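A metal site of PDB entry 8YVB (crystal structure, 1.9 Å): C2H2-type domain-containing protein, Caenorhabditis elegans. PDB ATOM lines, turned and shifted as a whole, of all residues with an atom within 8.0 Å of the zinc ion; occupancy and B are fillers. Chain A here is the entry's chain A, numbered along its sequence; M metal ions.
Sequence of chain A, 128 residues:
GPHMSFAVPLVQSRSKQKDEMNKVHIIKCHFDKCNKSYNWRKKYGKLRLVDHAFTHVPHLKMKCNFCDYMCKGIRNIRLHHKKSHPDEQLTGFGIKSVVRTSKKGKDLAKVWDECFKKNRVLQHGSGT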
ATOM      1  N   LYS A  28       1.214   8.274 -26.768  1.00  0.00           N
ATOM      2  CA  LYS A  28       0.297   7.545 -27.631  1.00  0.00           C
ATOM      3  C   LYS A  28      -1.082   7.452 -26.988  1.00  0.00           C
ATOM      4  O   LYS A  28      -1.197   7.226 -25.780  1.00  0.00           O
ATOM      5  CB  LYS A  28       0.819   6.133 -27.927  1.00  0.00           C
ATOM      6  CG  LYS A  28       2.055   6.104 -28.814  1.00  0.00           C
ATOM      7  CD  LYS A  28       2.422   4.682 -29.174  1.00  0.00           C
ATOM      8  CE  LYS A  28       3.583   4.642 -30.160  1.00  0.00           C
ATOM      9  NZ  LYS A  28       3.858   3.259 -30.636  1.00  0.00           N
ATOM     10  N   CYS A  29      -2.114   7.624 -27.806  1.00  0.00           N
ATOM     11  CA  CYS A  29      -3.473   7.402 -27.357  1.00  0.00           C
ATOM     12  C   CYS A  29      -3.815   5.920 -27.470  1.00  0.00           C
ATOM     13  O   CYS A  29      -3.611   5.313 -28.524  1.00  0.00           O
ATOM     14  CB  CYS A  29      -4.463   8.231 -28.168  1.00  0.00           C
ATOM     15  SG  CYS A  29      -6.183   7.968 -27.694  1.00  0.00           S
ATOM     16  N   HIS A  30      -4.322   5.342 -26.386  1.00  0.00           N
ATOM     17  CA  HIS A  30      -4.626   3.923 -26.328  1.00  0.00           C
ATOM     18  C   HIS A  30      -6.118   3.633 -26.484  1.00  0.00           C
ATOM     19  O   HIS A  30      -6.543   2.494 -26.240  1.00  0.00           O
ATOM     20  CB  HIS A  30      -4.108   3.314 -25.025  1.00  0.00           C
ATOM     21  CG  HIS A  30      -2.612   3.360 -24.900  1.00  0.00           C
ATOM     22  ND1 HIS A  30      -1.809   2.277 -25.144  1.00  0.00           N
ATOM     23  CD2 HIS A  30      -1.783   4.373 -24.543  1.00  0.00           C
ATOM     24  CE1 HIS A  30      -0.544   2.609 -24.944  1.00  0.00           C
ATOM     25  NE2 HIS A  30      -0.503   3.872 -24.577  1.00  0.00           N
ATOM     26  N   PHE A  31      -6.918   4.622 -26.870  1.00  0.00           N
ATOM     27  CA  PHE A  31      -8.338   4.364 -27.092  1.00  0.00           C
ATOM     28  C   PHE A  31      -8.502   3.396 -28.252  1.00  0.00           C
ATOM     29  O   PHE A  31      -7.639   3.283 -29.138  1.00  0.00           O
ATOM     30  CB  PHE A  31      -9.085   5.666 -27.390  1.00  0.00           C
ATOM     31  CG  PHE A  31     -10.567   5.558 -27.200  1.00  0.00           C
ATOM     32  CD1 PHE A  31     -11.137   5.758 -25.952  1.00  0.00           C
ATOM     33  CD2 PHE A  31     -11.398   5.254 -28.261  1.00  0.00           C
ATOM     34  CE1 PHE A  31     -12.512   5.651 -25.770  1.00  0.00           C
ATOM     35  CE2 PHE A  31     -12.771   5.145 -28.088  1.00  0.00           C
ATOM     36  CZ  PHE A  31     -13.327   5.350 -26.839  1.00  0.00           C
ATOM     37  N   ASP A  32      -9.616   2.670 -28.240  1.00  0.00           N
ATOM     38  CA  ASP A  32      -9.862   1.611 -29.215  1.00  0.00           C
ATOM     39  C   ASP A  32      -9.787   2.164 -30.644  1.00  0.00           C
ATOM     40  O   ASP A  32     -10.464   3.144 -30.968  1.00  0.00           O
ATOM     41  CB  ASP A  32     -11.214   0.973 -28.962  1.00  0.00           C
ATOM     42  CG  ASP A  32     -11.366  -0.373 -29.650  1.00  0.00           C
ATOM     43  OD1 ASP A  32     -10.919  -1.394 -29.081  1.00  0.00           O
ATOM     44  OD2 ASP A  32     -11.934  -0.409 -30.753  1.00  0.00           O
ATOM     45  N   LYS A  33      -8.933   1.546 -31.463  1.00  0.00           N
ATOM     46  CA  LYS A  33      -8.780   1.846 -32.883  1.00  0.00           C
ATOM     47  C   LYS A  33      -8.230   3.247 -33.146  1.00  0.00           C
ATOM     48  O   LYS A  33      -8.413   3.785 -34.248  1.00  0.00           O
ATOM     49  CB  LYS A  33     -10.087   1.656 -33.647  1.00  0.00           C
ATOM     50  CG  LYS A  33     -10.594   0.216 -33.661  1.00  0.00           C
ATOM     51  CD  LYS A  33     -11.912   0.112 -34.408  1.00  0.00           C
ATOM     52  CE  LYS A  33     -11.773   0.598 -35.847  1.00  0.00           C
ATOM     53  NZ  LYS A  33     -13.038   0.419 -36.616  1.00  0.00           N
ATOM     54  N   CYS A  34      -7.548   3.859 -32.188  1.00  0.00           N
ATOM     55  CA  CYS A  34      -6.979   5.182 -32.374  1.00  0.00           C
ATOM     56  C   CYS A  34      -5.457   5.070 -32.466  1.00  0.00           C
ATOM     57  O   CYS A  34      -4.824   4.436 -31.628  1.00  0.00           O
ATOM     58  CB  CYS A  34      -7.358   6.127 -31.236  1.00  0.00           C
ATOM     59  SG  CYS A  34      -6.816   7.808 -31.542  1.00  0.00           S
ATOM     60  N   ASN A  35      -4.886   5.703 -33.496  1.00  0.00           N
ATOM     61  CA  ASN A  35      -3.450   5.705 -33.722  1.00  0.00           C
ATOM     62  C   ASN A  35      -2.827   7.081 -33.528  1.00  0.00           C
ATOM     63  O   ASN A  35      -1.754   7.365 -34.068  1.00  0.00           O
ATOM     64  CB  ASN A  35      -3.126   5.179 -35.119  1.00  0.00           C
ATOM     65  CG  ASN A  35      -3.647   3.768 -35.355  1.00  0.00           C
ATOM     66  OD1 ASN A  35      -3.973   3.056 -34.407  1.00  0.00           O
ATOM     67  ND2 ASN A  35      -3.730   3.365 -36.613  1.00  0.00           N
ATOM     68  N   LYS A  36      -3.485   7.942 -32.759  1.00  0.00           N
ATOM     69  CA  LYS A  36      -2.967   9.284 -32.538  1.00  0.00           C
ATOM     70  C   LYS A  36      -1.750   9.236 -31.626  1.00  0.00           C
ATOM     71  O   LYS A  36      -1.693   8.456 -30.679  1.00  0.00           O
ATOM     72  CB  LYS A  36      -4.049  10.175 -31.936  1.00  0.00           C
ATOM     73  CG  LYS A  36      -3.608  11.615 -31.694  1.00  0.00           C
ATOM     74  CD  LYS A  36      -3.394  12.364 -33.005  1.00  0.00           C
ATOM     75  CE  LYS A  36      -4.721  12.767 -33.633  1.00  0.00           C
ATOM     76  NZ  LYS A  36      -4.532  13.816 -34.679  1.00  0.00           N
ATOM     77  N   SER A  37      -0.767  10.086 -31.932  1.00  0.00           N
ATOM     78  CA  SER A  37       0.425  10.217 -31.115  1.00  0.00           C
ATOM     79  C   SER A  37       0.863  11.667 -31.120  1.00  0.00           C
ATOM     80  O   SER A  37       0.608  12.409 -32.080  1.00  0.00           O
ATOM     81  CB  SER A  37       1.559   9.314 -31.617  1.00  0.00           C
ATOM     82  OG  SER A  37       1.994   9.707 -32.901  1.00  0.00           O
ATOM     83  N   TYR A  38       1.517  12.086 -30.033  1.00  0.00           N
ATOM     84  CA  TYR A  38       1.956  13.471 -29.862  1.00  0.00           C
ATOM     85  C   TYR A  38       3.403  13.513 -29.398  1.00  0.00           C
ATOM     86  O   TYR A  38       3.822  12.716 -28.555  1.00  0.00           O
ATOM     87  CB  TYR A  38       1.078  14.209 -28.847  1.00  0.00           C
ATOM     88  CG  TYR A  38      -0.364  14.420 -29.260  1.00  0.00           C
ATOM     89  CD1 TYR A  38      -0.722  15.458 -30.099  1.00  0.00           C
ATOM     90  CD2 TYR A  38      -1.364  13.567 -28.808  1.00  0.00           C
ATOM     91  CE1 TYR A  38      -2.032  15.653 -30.478  1.00  0.00           C
ATOM     92  CE2 TYR A  38      -2.681  13.756 -29.177  1.00  0.00           C
ATOM     93  CZ  TYR A  38      -3.013  14.804 -30.012  1.00  0.00           C
ATOM     94  OH  TYR A  38      -4.319  14.987 -30.387  1.00  0.00           O
ATOM     95  N   LEU A  49      -3.476  16.955 -24.743  1.00  0.00           N
ATOM     96  CA  LEU A  49      -3.821  15.567 -24.459  1.00  0.00           C
ATOM     97  C   LEU A  49      -5.251  15.434 -23.954  1.00  0.00           C
ATOM     98  O   LEU A  49      -5.985  14.541 -24.395  1.00  0.00           O
ATOM     99  CB  LEU A  49      -2.834  14.984 -23.448  1.00  0.00           C
ATOM    100  CG  LEU A  49      -1.368  15.046 -23.852  1.00  0.00           C
ATOM    101  CD1 LEU A  49      -0.488  14.423 -22.782  1.00  0.00           C
ATOM    102  CD2 LEU A  49      -1.152  14.366 -25.202  1.00  0.00           C
ATOM    103  N   HIS A  52      -7.672  15.868 -26.805  1.00  0.00           N
ATOM    104  CA  HIS A  52      -7.767  14.692 -27.673  1.00  0.00           C
ATOM    105  C   HIS A  52      -8.599  13.590 -27.034  1.00  0.00           C
ATOM    106  O   HIS A  52      -9.375  12.917 -27.732  1.00  0.00           O
ATOM    107  CB  HIS A  52      -6.380  14.137 -28.018  1.00  0.00           C
ATOM    108  CG  HIS A  52      -6.449  12.898 -28.842  1.00  0.00           C
ATOM    109  ND1 HIS A  52      -6.825  12.913 -30.169  1.00  0.00           N
ATOM    110  CD2 HIS A  52      -6.260  11.598 -28.523  1.00  0.00           C
ATOM    111  CE1 HIS A  52      -6.833  11.676 -30.631  1.00  0.00           C
ATOM    112  NE2 HIS A  52      -6.492  10.859 -29.652  1.00  0.00           N
ATOM    113  N   ALA A  53      -8.441  13.375 -25.736  1.00  0.00           N
ATOM    114  CA  ALA A  53      -9.257  12.375 -25.045  1.00  0.00           C
ATOM    115  C   ALA A  53     -10.731  12.700 -25.178  1.00  0.00           C
ATOM    116  O   ALA A  53     -11.570  11.802 -25.323  1.00  0.00           O
ATOM    117  CB  ALA A  53      -8.847  12.283 -23.584  1.00  0.00           C
ATOM    118  N   PHE A  54     -11.076  13.995 -25.150  1.00  0.00           N
ATOM    119  CA  PHE A  54     -12.460  14.415 -25.255  1.00  0.00           C
ATOM    120  C   PHE A  54     -13.062  14.153 -26.624  1.00  0.00           C
ATOM    121  O   PHE A  54     -14.296  14.056 -26.741  1.00  0.00           O
ATOM    122  CB  PHE A  54     -12.591  15.899 -24.900  1.00  0.00           C
ATOM    123  CG  PHE A  54     -12.424  16.189 -23.436  1.00  0.00           C
ATOM    124  CD1 PHE A  54     -12.308  15.160 -22.517  1.00  0.00           C
ATOM    125  CD2 PHE A  54     -12.371  17.494 -22.982  1.00  0.00           C
ATOM    126  CE1 PHE A  54     -12.147  15.426 -21.164  1.00  0.00           C
ATOM    127  CE2 PHE A  54     -12.215  17.772 -21.633  1.00  0.00           C
ATOM    128  CZ  PHE A  54     -12.101  16.732 -20.722  1.00  0.00           C
ATOM    129  N   THR A  55     -12.240  14.026 -27.675  1.00  0.00           N
ATOM    130  CA  THR A  55     -12.781  13.664 -28.983  1.00  0.00           C
ATOM    131  C   THR A  55     -13.321  12.229 -28.995  1.00  0.00           C
ATOM    132  O   THR A  55     -14.060  11.877 -29.916  1.00  0.00           O
ATOM    133  CB  THR A  55     -11.708  13.811 -30.070  1.00  0.00           C
ATOM    134  OG1 THR A  55     -10.690  12.819 -29.887  1.00  0.00           O
ATOM    135  CG2 THR A  55     -11.086  15.198 -30.027  1.00  0.00           C
ATOM    136  N   HIS A  56     -12.958  11.413 -28.012  1.00  0.00           N
ATOM    137  CA  HIS A  56     -13.486  10.061 -27.884  1.00  0.00           C
ATOM    138  C   HIS A  56     -14.736   9.992 -27.016  1.00  0.00           C
ATOM    139  O   HIS A  56     -15.219   8.884 -26.762  1.00  0.00           O
ATOM    140  CB  HIS A  56     -12.410   9.129 -27.322  1.00  0.00           C
ATOM    141  CG  HIS A  56     -11.224   8.953 -28.225  1.00  0.00           C
ATOM    142  ND1 HIS A  56     -11.319   8.377 -29.472  1.00  0.00           N
ATOM    143  CD2 HIS A  56      -9.915   9.281 -28.057  1.00  0.00           C
ATOM    144  CE1 HIS A  56     -10.127   8.350 -30.031  1.00  0.00           C
ATOM    145  NE2 HIS A  56      -9.260   8.896 -29.194  1.00  0.00           N
ATOM    146  N   VAL A 111     -12.354   8.473 -19.658  1.00  0.00           N
ATOM    147  CA  VAL A 111     -11.838   8.474 -21.023  1.00  0.00           C
ATOM    148  C   VAL A 111     -10.378   8.890 -21.044  1.00  0.00           C
ATOM    149  O   VAL A 111      -9.610   8.433 -21.905  1.00  0.00           O
ATOM    150  CB  VAL A 111     -12.708   9.363 -21.939  1.00  0.00           C
ATOM    151  CG1 VAL A 111     -12.466  10.830 -21.654  1.00  0.00           C
ATOM    152  CG2 VAL A 111     -12.417   9.047 -23.399  1.00  0.00           C
ATOM    153  N   GLU A 114      -8.509   5.701 -20.233  1.00  0.00           N
ATOM    154  CA  GLU A 114      -8.529   4.808 -21.379  1.00  0.00           C
ATOM    155  C   GLU A 114      -7.560   5.255 -22.472  1.00  0.00           C
ATOM    156  O   GLU A 114      -6.996   4.416 -23.173  1.00  0.00           O
ATOM    157  CB  GLU A 114      -9.949   4.714 -21.951  1.00  0.00           C
ATOM    158  CG  GLU A 114     -10.960   4.050 -21.022  1.00  0.00           C
ATOM    159  CD  GLU A 114     -12.358   4.022 -21.606  1.00  0.00           C
ATOM    160  OE1 GLU A 114     -12.550   4.550 -22.730  1.00  0.00           O
ATOM    161  OE2 GLU A 114     -13.268   3.468 -20.959  1.00  0.00           O
ATOM    162  N   CYS A 115      -7.349   6.562 -22.608  1.00  0.00           N
ATOM    163  CA  CYS A 115      -6.514   7.093 -23.668  1.00  0.00           C
ATOM    164  C   CYS A 115      -5.036   7.161 -23.299  1.00  0.00           C
ATOM    165  O   CYS A 115      -4.182   6.731 -24.072  1.00  0.00           O
ATOM    166  CB  CYS A 115      -7.008   8.501 -24.063  1.00  0.00           C
ATOM    167  SG  CYS A 115      -8.615   8.544 -24.883  1.00  0.00           S
ATOM    168  N   PHE A 116      -4.709   7.691 -22.115  1.00  0.00           N
ATOM    169  CA  PHE A 116      -3.345   8.097 -21.838  1.00  0.00           C
ATOM    170  C   PHE A 116      -2.739   7.542 -20.551  1.00  0.00           C
ATOM    171  O   PHE A 116      -1.557   7.811 -20.291  1.00  0.00           O
ATOM    172  CB  PHE A 116      -3.241   9.630 -21.803  1.00  0.00           C
ATOM    173  CG  PHE A 116      -3.529  10.280 -23.117  1.00  0.00           C
ATOM    174  CD1 PHE A 116      -2.676  10.098 -24.199  1.00  0.00           C
ATOM    175  CD2 PHE A 116      -4.639  11.084 -23.282  1.00  0.00           C
ATOM    176  CE1 PHE A 116      -2.932  10.690 -25.417  1.00  0.00           C
ATOM    177  CE2 PHE A 116      -4.900  11.689 -24.504  1.00  0.00           C
ATOM    178  CZ  PHE A 116      -4.049  11.488 -25.571  1.00  0.00           C
HETATM  179 ZN    ZN M   1      -7.282   8.832 -29.481  1.00  0.00          ZN
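O of His 52 sits at hydrogen-bond distance from OG1 of Thr 55, at 2.5 Å. ND1 of His 52 lies close to OH of Tyr 38. The side-chain sulfur (SG) of Cys 29 sits close to the backbone NH (N) of Phe 31 (3.5 Å). The backbone NH of Cys 29 lies within hydrogen-bond range of the backbone carbonyl oxygen of Lys 36 (3.0 Å). SG of Cys 29 sits close to SG of Cys 115, 3.8 Å away. The side-chain sulfur (SG) of Cys 34 sits close to the backbone NH (N) of Lys 36, 3.5 Å away.
The zinc ion is bound by a ring nitrogen (NE2) of His 56 (2.0 Å), a ring nitrogen (NE2) of His 52 (2.2 Å), the side-chain sulfur (SG) of Cys 29 (2.3 Å) and the side-chain sulfur (SG) of Cys 34 (2.3 Å).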
